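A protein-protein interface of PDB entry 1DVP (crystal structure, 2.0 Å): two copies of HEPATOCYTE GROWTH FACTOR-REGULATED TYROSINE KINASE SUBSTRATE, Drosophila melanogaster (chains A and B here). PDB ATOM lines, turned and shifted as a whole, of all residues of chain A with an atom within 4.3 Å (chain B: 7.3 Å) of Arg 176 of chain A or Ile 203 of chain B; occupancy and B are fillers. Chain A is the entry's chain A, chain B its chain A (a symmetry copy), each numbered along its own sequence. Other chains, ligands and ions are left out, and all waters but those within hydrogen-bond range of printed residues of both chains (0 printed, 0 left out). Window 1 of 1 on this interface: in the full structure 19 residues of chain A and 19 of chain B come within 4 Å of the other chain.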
ATOM      1  N   PHE A 171      -3.874 -12.806   1.172  1.00  0.00           N
ATOM      2  CA  PHE A 171      -3.152 -11.731   1.814  1.00  0.00           C
ATOM      3  C   PHE A 171      -3.420 -11.801   3.303  1.00  0.00           C
ATOM      4  O   PHE A 171      -4.490 -12.172   3.704  1.00  0.00           O
ATOM      5  CB  PHE A 171      -3.625 -10.348   1.300  1.00  0.00           C
ATOM      6  CG  PHE A 171      -3.273 -10.080  -0.156  1.00  0.00           C
ATOM      7  CD1 PHE A 171      -4.263  -9.775  -1.069  1.00  0.00           C
ATOM      8  CD2 PHE A 171      -1.937 -10.168  -0.586  1.00  0.00           C
ATOM      9  CE1 PHE A 171      -3.969  -9.562  -2.382  1.00  0.00           C
ATOM     10  CE2 PHE A 171      -1.623  -9.957  -1.895  1.00  0.00           C
ATOM     11  CZ  PHE A 171      -2.627  -9.651  -2.823  1.00  0.00           C
ATOM     12  N   THR A 172      -2.430 -11.424   4.107  1.00  0.00           N
ATOM     13  CA  THR A 172      -2.553 -11.342   5.563  1.00  0.00           C
ATOM     14  C   THR A 172      -2.161  -9.917   5.913  1.00  0.00           C
ATOM     15  O   THR A 172      -1.931  -9.120   5.031  1.00  0.00           O
ATOM     16  CB  THR A 172      -1.590 -12.321   6.288  1.00  0.00           C
ATOM     17  OG1 THR A 172      -0.218 -12.020   5.943  1.00  0.00           O
ATOM     18  CG2 THR A 172      -1.918 -13.780   5.841  1.00  0.00           C
ATOM     19  N   THR A 174       0.546  -9.227   7.333  1.00  0.00           N
ATOM     20  CA  THR A 174       1.992  -9.201   7.069  1.00  0.00           C
ATOM     21  C   THR A 174       2.361  -9.482   5.573  1.00  0.00           C
ATOM     22  O   THR A 174       3.322  -8.947   5.057  1.00  0.00           O
ATOM     23  CB  THR A 174       2.687 -10.224   7.996  1.00  0.00           C
ATOM     24  OG1 THR A 174       2.459  -9.813   9.344  1.00  0.00           O
ATOM     25  CG2 THR A 174       4.222 -10.316   7.688  1.00  0.00           C
ATOM     26  N   ASN A 175       1.604 -10.329   4.889  1.00  0.00           N
ATOM     27  CA  ASN A 175       1.823 -10.670   3.477  1.00  0.00           C
ATOM     28  C   ASN A 175       0.763  -9.842   2.749  1.00  0.00           C
ATOM     29  O   ASN A 175      -0.217 -10.358   2.301  1.00  0.00           O
ATOM     30  CB  ASN A 175       1.606 -12.178   3.287  1.00  0.00           C
ATOM     31  CG  ASN A 175       2.127 -12.713   1.961  1.00  0.00           C
ATOM     32  OD1 ASN A 175       2.549 -11.972   1.103  1.00  0.00           O
ATOM     33  ND2 ASN A 175       2.080 -14.052   1.792  1.00  0.00           N
ATOM     34  N   ARG A 176       0.996  -8.537   2.658  1.00  0.00           N
ATOM     35  CA  ARG A 176       0.052  -7.580   2.099  1.00  0.00           C
ATOM     36  C   ARG A 176       0.096  -7.386   0.577  1.00  0.00           C
ATOM     37  O   ARG A 176       1.029  -7.815  -0.125  1.00  0.00           O
ATOM     38  CB  ARG A 176       0.267  -6.240   2.802  1.00  0.00           C
ATOM     39  CG  ARG A 176       1.651  -5.640   2.507  1.00  0.00           C
ATOM     40  CD  ARG A 176       1.803  -4.238   3.118  1.00  0.00           C
ATOM     41  NE  ARG A 176       3.156  -3.738   2.921  1.00  0.00           N
ATOM     42  CZ  ARG A 176       3.577  -2.938   1.964  1.00  0.00           C
ATOM     43  NH1 ARG A 176       2.757  -2.438   1.001  1.00  0.00           N
ATOM     44  NH2 ARG A 176       4.891  -2.680   1.947  1.00  0.00           N
ATOM     45  N   LYS A 177      -0.912  -6.685   0.079  1.00  0.00           N
ATOM     46  CA  LYS A 177      -1.031  -6.455  -1.346  1.00  0.00           C
ATOM     47  C   LYS A 177      -0.136  -5.360  -1.866  1.00  0.00           C
ATOM     48  O   LYS A 177       0.348  -4.486  -1.118  1.00  0.00           O
ATOM     49  CB  LYS A 177      -2.481  -6.143  -1.687  1.00  0.00           C
ATOM     50  CG  LYS A 177      -3.045  -4.968  -0.915  1.00  0.00           C
ATOM     51  CD  LYS A 177      -4.602  -4.892  -1.093  1.00  0.00           C
ATOM     52  CE  LYS A 177      -5.206  -6.271  -0.962  1.00  0.00           C
ATOM     53  NZ  LYS A 177      -5.631  -6.607   0.462  1.00  0.00           N
ATOM     54  N   HIS A 178       0.107  -5.446  -3.161  1.00  0.00           N
ATOM     55  CA  HIS A 178       0.931  -4.475  -3.856  1.00  0.00           C
ATOM     56  C   HIS A 178       0.325  -4.419  -5.237  1.00  0.00           C
ATOM     57  O   HIS A 178      -0.111  -5.469  -5.728  1.00  0.00           O
ATOM     58  CB  HIS A 178       2.384  -4.966  -3.999  1.00  0.00           C
ATOM     59  CG  HIS A 178       3.073  -5.240  -2.709  1.00  0.00           C
ATOM     60  ND1 HIS A 178       3.732  -4.259  -1.973  1.00  0.00           N
ATOM     61  CD2 HIS A 178       3.144  -6.386  -1.977  1.00  0.00           C
ATOM     62  CE1 HIS A 178       4.160  -4.793  -0.843  1.00  0.00           C
ATOM     63  NE2 HIS A 178       3.815  -6.077  -0.818  1.00  0.00           N
ATOM     64  N   PHE A 187      -1.108  -8.168  -6.128  1.00  0.00           N
ATOM     65  CA  PHE A 187      -0.265  -9.352  -6.012  1.00  0.00           C
ATOM     66  C   PHE A 187       0.502  -9.299  -4.687  1.00  0.00           C
ATOM     67  O   PHE A 187       0.600  -8.217  -4.035  1.00  0.00           O
ATOM     68  CB  PHE A 187       0.810  -9.354  -7.127  1.00  0.00           C
ATOM     69  CG  PHE A 187       0.256  -9.224  -8.531  1.00  0.00           C
ATOM     70  CD1 PHE A 187      -0.148  -7.989  -9.062  1.00  0.00           C
ATOM     71  CD2 PHE A 187       0.172 -10.348  -9.349  1.00  0.00           C
ATOM     72  CE1 PHE A 187      -0.630  -7.872 -10.388  1.00  0.00           C
ATOM     73  CE2 PHE A 187      -0.303 -10.260 -10.646  1.00  0.00           C
ATOM     74  CZ  PHE A 187      -0.715  -8.995 -11.181  1.00  0.00           C
ATOM     75  N   CYS A 188       1.052 -10.458  -4.313  1.00  0.00           N
ATOM     76  CA  CYS A 188       1.889 -10.573  -3.138  1.00  0.00           C
ATOM     77  C   CYS A 188       3.271  -9.989  -3.581  1.00  0.00           C
ATOM     78  O   CYS A 188       3.513  -9.723  -4.748  1.00  0.00           O
ATOM     79  CB  CYS A 188       2.075 -12.039  -2.715  1.00  0.00           C
ATOM     80  SG  CYS A 188       2.952 -13.048  -3.948  1.00  0.00           S
ATOM     81  N   TRP B  23       4.281  -1.429  15.041  1.00  0.00           N
ATOM     82  CA  TRP B  23       3.249  -1.955  14.147  1.00  0.00           C
ATOM     83  C   TRP B  23       3.572  -3.334  13.562  1.00  0.00           C
ATOM     84  O   TRP B  23       2.703  -4.193  13.474  1.00  0.00           O
ATOM     85  CB  TRP B  23       2.953  -0.934  13.054  1.00  0.00           C
ATOM     86  CG  TRP B  23       2.179   0.183  13.661  1.00  0.00           C
ATOM     87  CD1 TRP B  23       2.622   1.465  13.981  1.00  0.00           C
ATOM     88  CD2 TRP B  23       0.863   0.080  14.185  1.00  0.00           C
ATOM     89  NE1 TRP B  23       1.648   2.141  14.686  1.00  0.00           N
ATOM     90  CE2 TRP B  23       0.558   1.320  14.819  1.00  0.00           C
ATOM     91  CE3 TRP B  23      -0.102  -0.942  14.184  1.00  0.00           C
ATOM     92  CZ2 TRP B  23      -0.663   1.555  15.441  1.00  0.00           C
ATOM     93  CZ3 TRP B  23      -1.338  -0.693  14.816  1.00  0.00           C
ATOM     94  CH2 TRP B  23      -1.589   0.542  15.431  1.00  0.00           C
ATOM     95  N   LEU B  27       0.885  -6.315  13.919  1.00  0.00           N
ATOM     96  CA  LEU B  27       0.295  -6.930  12.754  1.00  0.00           C
ATOM     97  C   LEU B  27       0.585  -8.456  12.806  1.00  0.00           C
ATOM     98  O   LEU B  27      -0.255  -9.273  12.405  1.00  0.00           O
ATOM     99  CB  LEU B  27       0.841  -6.249  11.471  1.00  0.00           C
ATOM    100  CG  LEU B  27       0.384  -4.758  11.376  1.00  0.00           C
ATOM    101  CD1 LEU B  27       0.897  -4.109  10.103  1.00  0.00           C
ATOM    102  CD2 LEU B  27      -1.174  -4.677  11.468  1.00  0.00           C
ATOM    103  N   ASP B  31      -2.238 -11.556  12.778  1.00  0.00           N
ATOM    104  CA  ASP B  31      -2.149 -12.748  11.921  1.00  0.00           C
ATOM    105  C   ASP B  31      -2.109 -14.056  12.749  1.00  0.00           C
ATOM    106  O   ASP B  31      -2.791 -15.042  12.416  1.00  0.00           O
ATOM    107  CB  ASP B  31      -0.896 -12.667  11.030  1.00  0.00           C
ATOM    108  CG  ASP B  31      -1.087 -11.710   9.836  1.00  0.00           C
ATOM    109  OD1 ASP B  31      -2.260 -11.472   9.452  1.00  0.00           O
ATOM    110  OD2 ASP B  31      -0.074 -11.231   9.298  1.00  0.00           O
ATOM    111  N   THR B 154      -6.176  -2.054   6.720  1.00  0.00           N
ATOM    112  CA  THR B 154      -5.857  -2.541   5.369  1.00  0.00           C
ATOM    113  C   THR B 154      -5.980  -1.358   4.427  1.00  0.00           C
ATOM    114  O   THR B 154      -6.904  -0.550   4.554  1.00  0.00           O
ATOM    115  CB  THR B 154      -6.805  -3.703   4.887  1.00  0.00           C
ATOM    116  OG1 THR B 154      -6.604  -4.880   5.694  1.00  0.00           O
ATOM    117  CG2 THR B 154      -6.513  -4.051   3.423  1.00  0.00           C
ATOM    118  N   ALA B 155      -5.020  -1.244   3.519  1.00  0.00           N
ATOM    119  CA  ALA B 155      -4.989  -0.153   2.540  1.00  0.00           C
ATOM    120  C   ALA B 155      -6.252  -0.121   1.673  1.00  0.00           C
ATOM    121  O   ALA B 155      -6.634  -1.129   1.075  1.00  0.00           O
ATOM    122  CB  ALA B 155      -3.751  -0.292   1.655  1.00  0.00           C
ATOM    123  N   TRP B 158      -7.770   1.272  -4.774  1.00  0.00           N
ATOM    124  CA  TRP B 158      -7.307   2.399  -5.569  1.00  0.00           C
ATOM    125  C   TRP B 158      -8.232   2.760  -6.691  1.00  0.00           C
ATOM    126  O   TRP B 158      -8.378   1.994  -7.654  1.00  0.00           O
ATOM    127  CB  TRP B 158      -5.918   2.050  -6.088  1.00  0.00           C
ATOM    128  CG  TRP B 158      -5.016   1.812  -4.923  1.00  0.00           C
ATOM    129  CD1 TRP B 158      -5.400   1.480  -3.667  1.00  0.00           C
ATOM    130  CD2 TRP B 158      -3.614   2.044  -4.864  1.00  0.00           C
ATOM    131  NE1 TRP B 158      -4.330   1.514  -2.818  1.00  0.00           N
ATOM    132  CE2 TRP B 158      -3.218   1.856  -3.529  1.00  0.00           C
ATOM    133  CE3 TRP B 158      -2.661   2.399  -5.805  1.00  0.00           C
ATOM    134  CZ2 TRP B 158      -1.898   2.019  -3.100  1.00  0.00           C
ATOM    135  CZ3 TRP B 158      -1.290   2.577  -5.361  1.00  0.00           C
ATOM    136  CH2 TRP B 158      -0.954   2.384  -4.027  1.00  0.00           C
ATOM    137  N   ARG B 181      -1.428   6.527  -1.221  1.00  0.00           N
ATOM    138  CA  ARG B 181      -1.446   5.215  -0.565  1.00  0.00           C
ATOM    139  C   ARG B 181      -2.319   5.165   0.696  1.00  0.00           C
ATOM    140  O   ARG B 181      -2.589   4.082   1.177  1.00  0.00           O
ATOM    141  CB  ARG B 181      -0.023   4.805  -0.217  1.00  0.00           C
ATOM    142  CG  ARG B 181       0.702   4.225  -1.330  1.00  0.00           C
ATOM    143  CD  ARG B 181       0.968   5.176  -2.452  1.00  0.00           C
ATOM    144  NE  ARG B 181       1.940   4.563  -3.360  1.00  0.00           N
ATOM    145  CZ  ARG B 181       2.221   4.955  -4.594  1.00  0.00           C
ATOM    146  NH1 ARG B 181       1.617   5.993  -5.184  1.00  0.00           N
ATOM    147  NH2 ARG B 181       3.146   4.266  -5.265  1.00  0.00           N
ATOM    148  N   ASN B 182      -2.749   6.305   1.256  1.00  0.00           N
ATOM    149  CA  ASN B 182      -3.624   6.284   2.417  1.00  0.00           C
ATOM    150  C   ASN B 182      -5.111   6.195   2.060  1.00  0.00           C
ATOM    151  O   ASN B 182      -5.850   5.436   2.712  1.00  0.00           O
ATOM    152  CB  ASN B 182      -3.450   7.540   3.310  1.00  0.00           C
ATOM    153  CG  ASN B 182      -4.142   7.392   4.670  1.00  0.00           C
ATOM    154  OD1 ASN B 182      -4.947   8.247   5.080  1.00  0.00           O
ATOM    155  ND2 ASN B 182      -3.848   6.292   5.373  1.00  0.00           N
ATOM    156  N   CYS B 196       5.022   9.921   3.599  1.00  0.00           N
ATOM    157  CA  CYS B 196       5.139   9.538   4.998  1.00  0.00           C
ATOM    158  C   CYS B 196       4.860   8.049   5.125  1.00  0.00           C
ATOM    159  O   CYS B 196       4.327   7.405   4.201  1.00  0.00           O
ATOM    160  CB  CYS B 196       4.189  10.339   5.899  1.00  0.00           C
ATOM    161  SG  CYS B 196       2.440   9.981   5.703  1.00  0.00           S
ATOM    162  N   PRO B 197       5.268   7.467   6.266  1.00  0.00           N
ATOM    163  CA  PRO B 197       5.012   6.033   6.401  1.00  0.00           C
ATOM    164  C   PRO B 197       3.574   5.759   6.786  1.00  0.00           C
ATOM    165  O   PRO B 197       2.867   6.664   7.237  1.00  0.00           O
ATOM    166  CB  PRO B 197       6.044   5.592   7.459  1.00  0.00           C
ATOM    167  CG  PRO B 197       6.270   6.810   8.259  1.00  0.00           C
ATOM    168  CD  PRO B 197       6.264   7.937   7.240  1.00  0.00           C
ATOM    169  N   LEU B 198       3.103   4.537   6.549  1.00  0.00           N
ATOM    170  CA  LEU B 198       1.735   4.194   6.932  1.00  0.00           C
ATOM    171  C   LEU B 198       1.925   2.864   7.611  1.00  0.00           C
ATOM    172  O   LEU B 198       1.485   1.788   7.145  1.00  0.00           O
ATOM    173  CB  LEU B 198       0.861   4.087   5.701  1.00  0.00           C
ATOM    174  CG  LEU B 198       0.760   5.429   4.940  1.00  0.00           C
ATOM    175  CD1 LEU B 198       0.130   5.171   3.583  1.00  0.00           C
ATOM    176  CD2 LEU B 198      -0.063   6.426   5.722  1.00  0.00           C
ATOM    177  N   PRO B 199       2.574   2.933   8.766  1.00  0.00           N
ATOM    178  CA  PRO B 199       2.847   1.695   9.495  1.00  0.00           C
ATOM    179  C   PRO B 199       1.615   0.847   9.859  1.00  0.00           C
ATOM    180  O   PRO B 199       1.703  -0.372   9.987  1.00  0.00           O
ATOM    181  CB  PRO B 199       3.712   2.184  10.661  1.00  0.00           C
ATOM    182  CG  PRO B 199       3.175   3.594  10.921  1.00  0.00           C
ATOM    183  CD  PRO B 199       2.871   4.151   9.551  1.00  0.00           C
ATOM    184  N   LYS B 200       0.456   1.467   9.969  1.00  0.00           N
ATOM    185  CA  LYS B 200      -0.732   0.679  10.298  1.00  0.00           C
ATOM    186  C   LYS B 200      -1.187  -0.212   9.163  1.00  0.00           C
ATOM    187  O   LYS B 200      -1.957  -1.165   9.372  1.00  0.00           O
ATOM    188  CB  LYS B 200      -1.880   1.567  10.745  1.00  0.00           C
ATOM    189  CG  LYS B 200      -1.750   1.985  12.168  1.00  0.00           C
ATOM    190  CD  LYS B 200      -2.469   3.308  12.406  1.00  0.00           C
ATOM    191  CE  LYS B 200      -1.755   4.197  13.487  1.00  0.00           C
ATOM    192  NZ  LYS B 200      -0.646   5.033  12.889  1.00  0.00           N
ATOM    193  N   TYR B 201      -0.732   0.101   7.969  1.00  0.00           N
ATOM    194  CA  TYR B 201      -1.032  -0.714   6.812  1.00  0.00           C
ATOM    195  C   TYR B 201       0.160  -1.619   6.499  1.00  0.00           C
ATOM    196  O   TYR B 201       0.205  -2.202   5.428  1.00  0.00           O
ATOM    197  CB  TYR B 201      -1.265   0.127   5.544  1.00  0.00           C
ATOM    198  CG  TYR B 201      -2.467   1.017   5.554  1.00  0.00           C
ATOM    199  CD1 TYR B 201      -3.518   0.812   6.422  1.00  0.00           C
ATOM    200  CD2 TYR B 201      -2.555   2.063   4.628  1.00  0.00           C
ATOM    201  CE1 TYR B 201      -4.656   1.644   6.375  1.00  0.00           C
ATOM    202  CE2 TYR B 201      -3.643   2.864   4.564  1.00  0.00           C
ATOM    203  CZ  TYR B 201      -4.704   2.663   5.435  1.00  0.00           C
ATOM    204  OH  TYR B 201      -5.809   3.473   5.295  1.00  0.00           O
ATOM    205  N   GLY B 202       1.138  -1.677   7.408  1.00  0.00           N
ATOM    206  CA  GLY B 202       2.326  -2.515   7.209  1.00  0.00           C
ATOM    207  C   GLY B 202       3.331  -1.829   6.313  1.00  0.00           C
ATOM    208  O   GLY B 202       4.254  -2.469   5.792  1.00  0.00           O
ATOM    209  N   ILE B 203       3.188  -0.518   6.120  1.00  0.00           N
ATOM    210  CA  ILE B 203       4.141   0.162   5.252  1.00  0.00           C
ATOM    211  C   ILE B 203       5.057   1.050   6.099  1.00  0.00           C
ATOM    212  O   ILE B 203       4.653   2.112   6.532  1.00  0.00           O
ATOM    213  CB  ILE B 203       3.396   1.032   4.237  1.00  0.00           C
ATOM    214  CG1 ILE B 203       2.232   0.226   3.640  1.00  0.00           C
ATOM    215  CG2 ILE B 203       4.360   1.537   3.155  1.00  0.00           C
ATOM    216  CD1 ILE B 203       1.427   0.993   2.618  1.00  0.00           C
ATOM    217  N   GLU B 204       6.293   0.627   6.326  1.00  0.00           N
ATOM    218  CA  GLU B 204       7.203   1.402   7.173  1.00  0.00           C
ATOM    219  C   GLU B 204       7.928   2.519   6.419  1.00  0.00           C
ATOM    220  O   GLU B 204       8.219   3.563   6.987  1.00  0.00           O
ATOM    221  CB  GLU B 204       8.240   0.478   7.848  1.00  0.00           C
ATOM    222  CG  GLU B 204       7.660  -0.511   8.809  1.00  0.00           C
ATOM    223  CD  GLU B 204       7.230   0.121  10.122  1.00  0.00           C
ATOM    224  OE1 GLU B 204       8.057   0.821  10.755  1.00  0.00           O
ATOM    225  OE2 GLU B 204       6.069  -0.079  10.534  1.00  0.00           O
ATOM    226  N   LYS B 205       8.220   2.301   5.152  1.00  0.00           N
ATOM    227  CA  LYS B 205       8.874   3.328   4.345  1.00  0.00           C
ATOM    228  C   LYS B 205       7.892   4.479   4.020  1.00  0.00           C
ATOM    229  O   LYS B 205       6.667   4.316   4.046  1.00  0.00           O
ATOM    230  CB  LYS B 205       9.357   2.688   3.058  1.00  0.00           C
ATOM    231  CG  LYS B 205       8.220   2.371   2.068  1.00  0.00           C
ATOM    232  CD  LYS B 205       8.721   1.573   0.859  1.00  0.00           C
ATOM    233  CE  LYS B 205       9.861   2.263   0.173  1.00  0.00           C
ATOM    234  NZ  LYS B 205       9.363   3.152  -0.944  1.00  0.00           N
ATOM    235  N   GLU B 206       8.435   5.653   3.738  1.00  0.00           N
ATOM    236  CA  GLU B 206       7.617   6.806   3.408  1.00  0.00           C
ATOM    237  C   GLU B 206       7.112   6.623   1.981  1.00  0.00           C
ATOM    238  O   GLU B 206       7.906   6.404   1.075  1.00  0.00           O
ATOM    239  CB  GLU B 206       8.442   8.075   3.522  1.00  0.00           C
ATOM    240  CG  GLU B 206       8.593   8.482   4.965  1.00  0.00           C
ATOM    241  CD  GLU B 206       9.295   9.796   5.144  1.00  0.00           C
ATOM    242  OE1 GLU B 206       9.485  10.213   6.311  1.00  0.00           O
ATOM    243  OE2 GLU B 206       9.657  10.412   4.117  1.00  0.00           O
ATOM    244  N   VAL B 207       5.798   6.695   1.803  1.00  0.00           N
ATOM    245  CA  VAL B 207       5.188   6.519   0.504  1.00  0.00           C
ATOM    246  C   VAL B 207       4.362   7.786   0.140  1.00  0.00           C
ATOM    247  O   VAL B 207       4.044   8.613   0.994  1.00  0.00           O
ATOM    248  CB  VAL B 207       4.259   5.275   0.514  1.00  0.00           C
ATOM    249  CG1 VAL B 207       5.076   3.971   0.656  1.00  0.00           C
ATOM    250  CG2 VAL B 207       3.272   5.378   1.662  1.00  0.00           C
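OG1 of Thr 172 of chain A sits at hydrogen-bond distance from OD2 of Asp 31 of chain B, 3.4 Å away. The backbone NH of Thr 174 of chain A lies within hydrogen-bond range of the side-chain carboxylate of Asp 31 of chain B (2.9 Å). The backbone carbonyl oxygen (O) of Gly 202 of chain B sits at hydrogen-bond distance from the guanidinium group (NE) of Arg 176 of chain A (3.3 Å).
The side-chain hydroxyl of Thr 172 of chain A sits close to the backbone NH of Thr 174 of chain A, at 3.2 Å. The side-chain hydroxyl (OG1) of Thr 172 of chain A sits at hydrogen-bond distance from the backbone NH (N) of Asn 175 of chain A (2.7 Å). A ring nitrogen (NE2) of His 178 of chain A sits close to the backbone carbonyl oxygen (O) of Arg 176 of chain A (3.4 Å). The side-chain hydroxyl (OH) of Tyr 201 of chain B sits at hydrogen-bond distance from the backbone carbonyl oxygen (O) of Asn 182 of chain B. The backbone carbonyl oxygen (O) of Ile 203 of chain B is in hydrogen-bond range of the backbone NH (N) of Leu 198 of chain B (2.9 Å).
Among the printed residues, pairs that only touch across the chains: Arg 176 of chain A with Tyr 201 of chain B (3.5 Å) and Arg 176 of chain A with Ile 203 of chain B (3.8 Å).
Of chain B, only Tyr 201 (3.5 Å), Gly 202 (3.3 Å) and Ile 203 (3.8 Å) come within 4 Å of Arg 176 of chain A. Of the printed residues of chain A, Ile 203 of chain B touches Arg 176. Of the printed residues of chain A, Asp 31 of chain B touches Thr 172 and Thr 174. Of the printed residues of chain B, Thr 174 of chain A touches Asp 31 (2.9 Å). The nearest printed residue of chain A that does not touch Ile 203 of chain B is Lys 177 of chain A (6.7 Å).
Of the 20 printed residues of chain B, 4 touch a printed residue of chain A. Of the 9 printed residues of chain A, 3 touch a printed residue of chain B. Among the printed residues, 5 pairs touch across the chains. Among the printed residues, no Asp or Glu carboxylate lies within 4 Å of a Lys or Arg side-chain nitrogen of the other chain.
No position is printed for both chains. Of the 5 pairs that touch across the chains among the printed residues, none has its exchanged pair printed and touching as well.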
